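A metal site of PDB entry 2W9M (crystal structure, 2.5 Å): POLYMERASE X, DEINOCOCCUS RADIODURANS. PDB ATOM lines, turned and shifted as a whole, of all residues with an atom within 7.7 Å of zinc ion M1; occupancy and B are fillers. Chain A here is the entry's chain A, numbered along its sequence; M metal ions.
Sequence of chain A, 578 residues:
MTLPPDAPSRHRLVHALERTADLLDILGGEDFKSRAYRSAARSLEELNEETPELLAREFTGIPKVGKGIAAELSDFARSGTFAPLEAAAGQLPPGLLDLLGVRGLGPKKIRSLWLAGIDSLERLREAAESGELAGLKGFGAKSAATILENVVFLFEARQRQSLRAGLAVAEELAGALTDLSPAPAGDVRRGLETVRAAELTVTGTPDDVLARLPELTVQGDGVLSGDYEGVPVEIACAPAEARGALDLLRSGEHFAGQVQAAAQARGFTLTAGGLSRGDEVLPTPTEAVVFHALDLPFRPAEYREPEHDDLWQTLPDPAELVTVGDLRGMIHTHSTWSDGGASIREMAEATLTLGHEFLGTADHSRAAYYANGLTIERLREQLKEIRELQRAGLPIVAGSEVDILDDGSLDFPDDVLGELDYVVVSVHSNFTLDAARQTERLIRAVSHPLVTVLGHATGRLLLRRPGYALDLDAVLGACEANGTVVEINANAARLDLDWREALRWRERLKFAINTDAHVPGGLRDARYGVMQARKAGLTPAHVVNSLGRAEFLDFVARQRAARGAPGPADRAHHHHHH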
ATOM      1  N   LEU A  27     -11.234  12.828   8.435  1.00  0.00           N
ATOM      2  CA  LEU A  27     -11.616  11.976   7.311  1.00  0.00           C
ATOM      3  C   LEU A  27     -11.630  10.507   7.685  1.00  0.00           C
ATOM      4  O   LEU A  27     -12.570   9.786   7.367  1.00  0.00           O
ATOM      5  CB  LEU A  27     -10.672  12.213   6.123  1.00  0.00           C
ATOM      6  CG  LEU A  27     -10.381  13.684   5.790  1.00  0.00           C
ATOM      7  CD1 LEU A  27      -9.356  13.775   4.665  1.00  0.00           C
ATOM      8  CD2 LEU A  27     -11.646  14.441   5.407  1.00  0.00           C
ATOM      9  N   GLN A  91      -2.919  18.371   0.331  1.00  0.00           N
ATOM     10  CA  GLN A  91      -3.774  17.223  -0.003  1.00  0.00           C
ATOM     11  C   GLN A  91      -5.252  17.490   0.234  1.00  0.00           C
ATOM     12  O   GLN A  91      -6.100  17.016  -0.520  1.00  0.00           O
ATOM     13  CB  GLN A  91      -3.334  15.998   0.786  1.00  0.00           C
ATOM     14  CG  GLN A  91      -1.917  15.552   0.477  1.00  0.00           C
ATOM     15  CD  GLN A  91      -1.483  14.398   1.329  1.00  0.00           C
ATOM     16  OE1 GLN A  91      -2.316  13.655   1.852  1.00  0.00           O
ATOM     17  NE2 GLN A  91      -0.180  14.228   1.489  1.00  0.00           N
ATOM     18  N   LEU A  92      -5.545  18.248   1.289  1.00  0.00           N
ATOM     19  CA  LEU A  92      -6.927  18.506   1.676  1.00  0.00           C
ATOM     20  C   LEU A  92      -7.653  19.455   0.725  1.00  0.00           C
ATOM     21  O   LEU A  92      -7.015  20.308   0.081  1.00  0.00           O
ATOM     22  CB  LEU A  92      -6.975  19.045   3.110  1.00  0.00           C
ATOM     23  CG  LEU A  92      -6.569  18.016   4.174  1.00  0.00           C
ATOM     24  CD1 LEU A  92      -6.529  18.664   5.551  1.00  0.00           C
ATOM     25  CD2 LEU A  92      -7.507  16.811   4.176  1.00  0.00           C
ATOM     26  N   PRO A  93      -8.977  19.311   0.620  1.00  0.00           N
ATOM     27  CA  PRO A  93      -9.808  20.165  -0.233  1.00  0.00           C
ATOM     28  C   PRO A  93      -9.789  21.597   0.284  1.00  0.00           C
ATOM     29  O   PRO A  93      -9.719  21.807   1.488  1.00  0.00           O
ATOM     30  CB  PRO A  93     -11.212  19.577  -0.057  1.00  0.00           C
ATOM     31  CG  PRO A  93     -11.001  18.195   0.467  1.00  0.00           C
ATOM     32  CD  PRO A  93      -9.766  18.275   1.297  1.00  0.00           C
ATOM     33  N   PRO A  94      -9.880  22.576  -0.627  1.00  0.00           N
ATOM     34  CA  PRO A  94      -9.851  24.008  -0.283  1.00  0.00           C
ATOM     35  C   PRO A  94     -10.900  24.381   0.752  1.00  0.00           C
ATOM     36  O   PRO A  94     -10.612  25.131   1.676  1.00  0.00           O
ATOM     37  CB  PRO A  94     -10.183  24.686  -1.621  1.00  0.00           C
ATOM     38  CG  PRO A  94      -9.715  23.723  -2.648  1.00  0.00           C
ATOM     39  CD  PRO A  94      -9.989  22.361  -2.076  1.00  0.00           C
ATOM     40  N   TRP A 114     -19.119  18.021   6.980  1.00  0.00           N
ATOM     41  CA  TRP A 114     -18.692  17.384   5.733  1.00  0.00           C
ATOM     42  C   TRP A 114     -19.675  16.283   5.331  1.00  0.00           C
ATOM     43  O   TRP A 114     -20.110  16.230   4.180  1.00  0.00           O
ATOM     44  CB  TRP A 114     -17.273  16.805   5.885  1.00  0.00           C
ATOM     45  CG  TRP A 114     -16.517  16.731   4.600  1.00  0.00           C
ATOM     46  CD1 TRP A 114     -16.281  15.605   3.852  1.00  0.00           C
ATOM     47  CD2 TRP A 114     -15.904  17.819   3.899  1.00  0.00           C
ATOM     48  NE1 TRP A 114     -15.547  15.929   2.734  1.00  0.00           N
ATOM     49  CE2 TRP A 114     -15.303  17.281   2.743  1.00  0.00           C
ATOM     50  CE3 TRP A 114     -15.799  19.186   4.132  1.00  0.00           C
ATOM     51  CZ2 TRP A 114     -14.611  18.070   1.820  1.00  0.00           C
ATOM     52  CZ3 TRP A 114     -15.109  19.974   3.219  1.00  0.00           C
ATOM     53  CH2 TRP A 114     -14.522  19.413   2.077  1.00  0.00           C
ATOM     54  N   HIS A 332     -14.104  13.261 -12.297  1.00  0.00           N
ATOM     55  CA  HIS A 332     -13.260  13.748 -11.222  1.00  0.00           C
ATOM     56  C   HIS A 332     -14.088  14.205 -10.018  1.00  0.00           C
ATOM     57  O   HIS A 332     -14.147  15.378  -9.684  1.00  0.00           O
ATOM     58  CB  HIS A 332     -12.335  14.859 -11.717  1.00  0.00           C
ATOM     59  CG  HIS A 332     -11.301  15.271 -10.712  1.00  0.00           C
ATOM     60  ND1 HIS A 332     -10.547  16.416 -10.851  1.00  0.00           N
ATOM     61  CD2 HIS A 332     -10.910  14.703  -9.551  1.00  0.00           C
ATOM     62  CE1 HIS A 332      -9.730  16.527  -9.825  1.00  0.00           C
ATOM     63  NE2 HIS A 332      -9.931  15.496  -9.018  1.00  0.00           N
ATOM     64  N   HIS A 334     -15.176  13.015  -5.793  1.00  0.00           N
ATOM     65  CA  HIS A 334     -14.663  12.253  -4.653  1.00  0.00           C
ATOM     66  C   HIS A 334     -15.787  11.675  -3.794  1.00  0.00           C
ATOM     67  O   HIS A 334     -16.871  12.250  -3.711  1.00  0.00           O
ATOM     68  CB  HIS A 334     -13.714  13.093  -3.807  1.00  0.00           C
ATOM     69  CG  HIS A 334     -12.456  13.468  -4.521  1.00  0.00           C
ATOM     70  ND1 HIS A 334     -11.254  12.817  -4.318  1.00  0.00           N
ATOM     71  CD2 HIS A 334     -12.208  14.418  -5.457  1.00  0.00           C
ATOM     72  CE1 HIS A 334     -10.322  13.345  -5.086  1.00  0.00           C
ATOM     73  NE2 HIS A 334     -10.884  14.327  -5.795  1.00  0.00           N
ATOM     74  N   SER A 338     -12.452   8.152  -0.193  1.00  0.00           N
ATOM     75  CA  SER A 338     -11.299   9.026  -0.098  1.00  0.00           C
ATOM     76  C   SER A 338     -11.554  10.095   0.977  1.00  0.00           C
ATOM     77  O   SER A 338     -11.720   9.778   2.160  1.00  0.00           O
ATOM     78  CB  SER A 338     -11.041   9.693  -1.441  1.00  0.00           C
ATOM     79  OG  SER A 338      -9.698  10.104  -1.576  1.00  0.00           O
ATOM     80  N   ASP A 339     -11.579  11.349   0.558  1.00  0.00           N
ATOM     81  CA  ASP A 339     -11.884  12.449   1.464  1.00  0.00           C
ATOM     82  C   ASP A 339     -13.185  13.164   1.098  1.00  0.00           C
ATOM     83  O   ASP A 339     -13.359  14.338   1.391  1.00  0.00           O
ATOM     84  CB  ASP A 339     -10.718  13.441   1.530  1.00  0.00           C
ATOM     85  CG  ASP A 339     -10.451  14.125   0.201  1.00  0.00           C
ATOM     86  OD1 ASP A 339     -10.995  13.669  -0.834  1.00  0.00           O
ATOM     87  OD2 ASP A 339      -9.698  15.127   0.182  1.00  0.00           O
ATOM     88  N   GLY A 340     -14.100  12.439   0.454  1.00  0.00           N
ATOM     89  CA  GLY A 340     -15.418  12.957   0.165  1.00  0.00           C
ATOM     90  C   GLY A 340     -16.357  12.763   1.340  1.00  0.00           C
ATOM     91  O   GLY A 340     -15.994  12.143   2.343  1.00  0.00           O
ATOM     92  N   ALA A 362     -13.199   9.283  -8.996  1.00  0.00           N
ATOM     93  CA  ALA A 362     -11.796   9.709  -9.004  1.00  0.00           C
ATOM     94  C   ALA A 362     -11.249  10.070  -7.613  1.00  0.00           C
ATOM     95  O   ALA A 362     -10.886  11.213  -7.371  1.00  0.00           O
ATOM     96  CB  ALA A 362     -11.590  10.869  -9.963  1.00  0.00           C
ATOM     97  N   ASP A 363     -11.194   9.087  -6.730  1.00  0.00           N
ATOM     98  CA  ASP A 363     -10.671   9.304  -5.379  1.00  0.00           C
ATOM     99  C   ASP A 363      -9.144   9.299  -5.386  1.00  0.00           C
ATOM    100  O   ASP A 363      -8.525   8.824  -6.333  1.00  0.00           O
ATOM    101  CB  ASP A 363     -11.236   8.239  -4.418  1.00  0.00           C
ATOM    102  CG  ASP A 363     -12.686   8.512  -4.042  1.00  0.00           C
ATOM    103  OD1 ASP A 363     -12.955   9.561  -3.427  1.00  0.00           O
ATOM    104  OD2 ASP A 363     -13.560   7.680  -4.377  1.00  0.00           O
ATOM    105  N   HIS A 364      -8.536   9.840  -4.335  1.00  0.00           N
ATOM    106  CA  HIS A 364      -7.075   9.937  -4.276  1.00  0.00           C
ATOM    107  C   HIS A 364      -6.444   8.573  -4.114  1.00  0.00           C
ATOM    108  O   HIS A 364      -7.119   7.574  -3.843  1.00  0.00           O
ATOM    109  CB  HIS A 364      -6.628  10.819  -3.103  1.00  0.00           C
ATOM    110  CG  HIS A 364      -7.274  12.158  -3.065  1.00  0.00           C
ATOM    111  ND1 HIS A 364      -6.768  13.254  -3.733  1.00  0.00           N
ATOM    112  CD2 HIS A 364      -8.402  12.577  -2.439  1.00  0.00           C
ATOM    113  CE1 HIS A 364      -7.558  14.292  -3.515  1.00  0.00           C
ATOM    114  NE2 HIS A 364      -8.553  13.908  -2.744  1.00  0.00           N
ATOM    115  N   ALA A 368      -1.567  10.368  -1.079  1.00  0.00           N
ATOM    116  CA  ALA A 368      -2.363  11.360  -0.376  1.00  0.00           C
ATOM    117  C   ALA A 368      -2.836  10.795   0.956  1.00  0.00           C
ATOM    118  O   ALA A 368      -3.986  10.406   1.099  1.00  0.00           O
ATOM    119  CB  ALA A 368      -3.548  11.802  -1.231  1.00  0.00           C
ATOM    120  N   ALA A 371      -5.558  12.673   3.085  1.00  0.00           N
ATOM    121  CA  ALA A 371      -6.833  12.756   2.378  1.00  0.00           C
ATOM    122  C   ALA A 371      -7.460  11.374   2.221  1.00  0.00           C
ATOM    123  O   ALA A 371      -8.348  11.179   1.395  1.00  0.00           O
ATOM    124  CB  ALA A 371      -6.647  13.424   1.042  1.00  0.00           C
ATOM    125  N   ASN A 372      -6.981  10.422   3.013  1.00  0.00           N
ATOM    126  CA  ASN A 372      -7.523   9.069   3.021  1.00  0.00           C
ATOM    127  C   ASN A 372      -7.417   8.382   1.665  1.00  0.00           C
ATOM    128  O   ASN A 372      -8.376   7.750   1.194  1.00  0.00           O
ATOM    129  CB  ASN A 372      -8.980   9.088   3.508  1.00  0.00           C
ATOM    130  CG  ASN A 372      -9.494   7.710   3.878  1.00  0.00           C
ATOM    131  OD1 ASN A 372      -8.760   6.874   4.417  1.00  0.00           O
ATOM    132  ND2 ASN A 372     -10.764   7.464   3.591  1.00  0.00           N
ATOM    133  N   GLU A 401      -7.711   9.636  -9.003  1.00  0.00           N
ATOM    134  CA  GLU A 401      -6.825  10.786  -9.086  1.00  0.00           C
ATOM    135  C   GLU A 401      -5.455  10.370  -8.584  1.00  0.00           C
ATOM    136  O   GLU A 401      -5.170  10.430  -7.386  1.00  0.00           O
ATOM    137  CB  GLU A 401      -7.349  11.975  -8.288  1.00  0.00           C
ATOM    138  CG  GLU A 401      -6.537  13.239  -8.540  1.00  0.00           C
ATOM    139  CD  GLU A 401      -7.009  14.428  -7.753  1.00  0.00           C
ATOM    140  OE1 GLU A 401      -8.011  14.283  -7.014  1.00  0.00           O
ATOM    141  OE2 GLU A 401      -6.375  15.503  -7.874  1.00  0.00           O
ATOM    142  N   HIS A 428      -0.081  16.911  -5.479  1.00  0.00           N
ATOM    143  CA  HIS A 428      -0.619  17.153  -4.155  1.00  0.00           C
ATOM    144  C   HIS A 428       0.503  17.168  -3.109  1.00  0.00           C
ATOM    145  O   HIS A 428       0.259  17.113  -1.896  1.00  0.00           O
ATOM    146  CB  HIS A 428      -1.651  16.089  -3.786  1.00  0.00           C
ATOM    147  CG  HIS A 428      -2.992  16.294  -4.421  1.00  0.00           C
ATOM    148  ND1 HIS A 428      -3.806  17.367  -4.109  1.00  0.00           N
ATOM    149  CD2 HIS A 428      -3.670  15.555  -5.323  1.00  0.00           C
ATOM    150  CE1 HIS A 428      -4.921  17.281  -4.815  1.00  0.00           C
ATOM    151  NE2 HIS A 428      -4.855  16.193  -5.567  1.00  0.00           N
ATOM    152  N   ARG A 494     -10.296  27.009  -7.039  1.00  0.00           N
ATOM    153  CA  ARG A 494      -9.252  26.640  -7.982  1.00  0.00           C
ATOM    154  C   ARG A 494      -9.358  27.398  -9.305  1.00  0.00           C
ATOM    155  O   ARG A 494      -8.472  28.178  -9.647  1.00  0.00           O
ATOM    156  CB  ARG A 494      -9.234  25.126  -8.218  1.00  0.00           C
ATOM    157  CG  ARG A 494      -8.808  24.343  -6.995  1.00  0.00           C
ATOM    158  CD  ARG A 494      -8.779  22.848  -7.287  1.00  0.00           C
ATOM    159  NE  ARG A 494      -8.491  22.055  -6.091  1.00  0.00           N
ATOM    160  CZ  ARG A 494      -7.278  21.888  -5.585  1.00  0.00           C
ATOM    161  NH1 ARG A 494      -6.225  22.467  -6.147  1.00  0.00           N
ATOM    162  NH2 ARG A 494      -7.121  21.140  -4.499  1.00  0.00           N
ATOM    163  N   ASP A 516     -14.567  18.498  -9.309  1.00  0.00           N
ATOM    164  CA  ASP A 516     -13.756  18.014  -8.190  1.00  0.00           C
ATOM    165  C   ASP A 516     -14.600  17.962  -6.922  1.00  0.00           C
ATOM    166  O   ASP A 516     -14.110  18.226  -5.827  1.00  0.00           O
ATOM    167  CB  ASP A 516     -12.539  18.917  -7.985  1.00  0.00           C
ATOM    168  CG  ASP A 516     -11.415  18.223  -7.237  1.00  0.00           C
ATOM    169  OD1 ASP A 516     -11.634  17.091  -6.770  1.00  0.00           O
ATOM    170  OD2 ASP A 516     -10.316  18.811  -7.118  1.00  0.00           O
ATOM    171  N   ALA A 517     -15.870  17.600  -7.074  1.00  0.00           N
ATOM    172  CA  ALA A 517     -16.818  17.568  -5.955  1.00  0.00           C
ATOM    173  C   ALA A 517     -16.417  16.602  -4.840  1.00  0.00           C
ATOM    174  O   ALA A 517     -16.162  15.415  -5.079  1.00  0.00           O
ATOM    175  CB  ALA A 517     -18.219  17.233  -6.458  1.00  0.00           C
ATOM    176  N   HIS A 518     -16.361  17.102  -3.610  1.00  0.00           N
ATOM    177  CA  HIS A 518     -16.121  16.266  -2.450  1.00  0.00           C
ATOM    178  C   HIS A 518     -17.421  16.016  -1.682  1.00  0.00           C
ATOM    179  O   HIS A 518     -17.432  15.373  -0.639  1.00  0.00           O
ATOM    180  CB  HIS A 518     -15.075  16.908  -1.539  1.00  0.00           C
ATOM    181  CG  HIS A 518     -13.682  16.784  -2.055  1.00  0.00           C
ATOM    182  ND1 HIS A 518     -13.213  17.516  -3.122  1.00  0.00           N
ATOM    183  CD2 HIS A 518     -12.654  15.996  -1.670  1.00  0.00           C
ATOM    184  CE1 HIS A 518     -11.962  17.197  -3.368  1.00  0.00           C
ATOM    185  NE2 HIS A 518     -11.586  16.266  -2.499  1.00  0.00           N
HETATM  186 ZN    ZN M   1      -9.689  15.498  -2.073  1.00  0.00          ZN
HETATM  187 ZN    ZN M   2      -9.552  15.892  -6.817  1.00  0.00          ZN
HETATM  188 ZN    ZN M   3      -6.848  17.135  -6.609  1.00  0.00          ZN
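A ring nitrogen (NE2) of His 364 is bound to zinc ion M1.
NE2 of His 518 binds zinc ion M1 (2.1 Å).
The side-chain carboxylate (OD2) of Asp 339 is bound to zinc ion M1.
Zinc ion M1 is bound by the side-chain carboxylate (OD1) of Asp 339.
A ring nitrogen (NE2) of His 364 lies close to a ring nitrogen (ND1) of His 334, at 3.3 Å.
The backbone NH (N) of His 364 lies close to the side-chain hydroxyl (OG) of Ser 338 (3.0 Å).
O of Asp 516 sits at hydrogen-bond distance from ND1 of His 518, 2.9 Å away.
O of Ala 371 lies close to N of Asp 339, 3.3 Å away.
The backbone carbonyl oxygen (O) of Asp 339 is in hydrogen-bond range of the indole nitrogen (NE1) of Trp 114 (3.0 Å).
The backbone carbonyl oxygen (O) of Ala 362 lies close to a ring nitrogen (ND1) of His 334.
N of His 334 lies within hydrogen-bond range of O of Ala 517.
Residues that only touch zinc ion M1: Pro 93 (3.9 Å) and His 334 (3.8 Å).
Of the 23 residues printed, 5 come within 4 Å of zinc ion M1.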
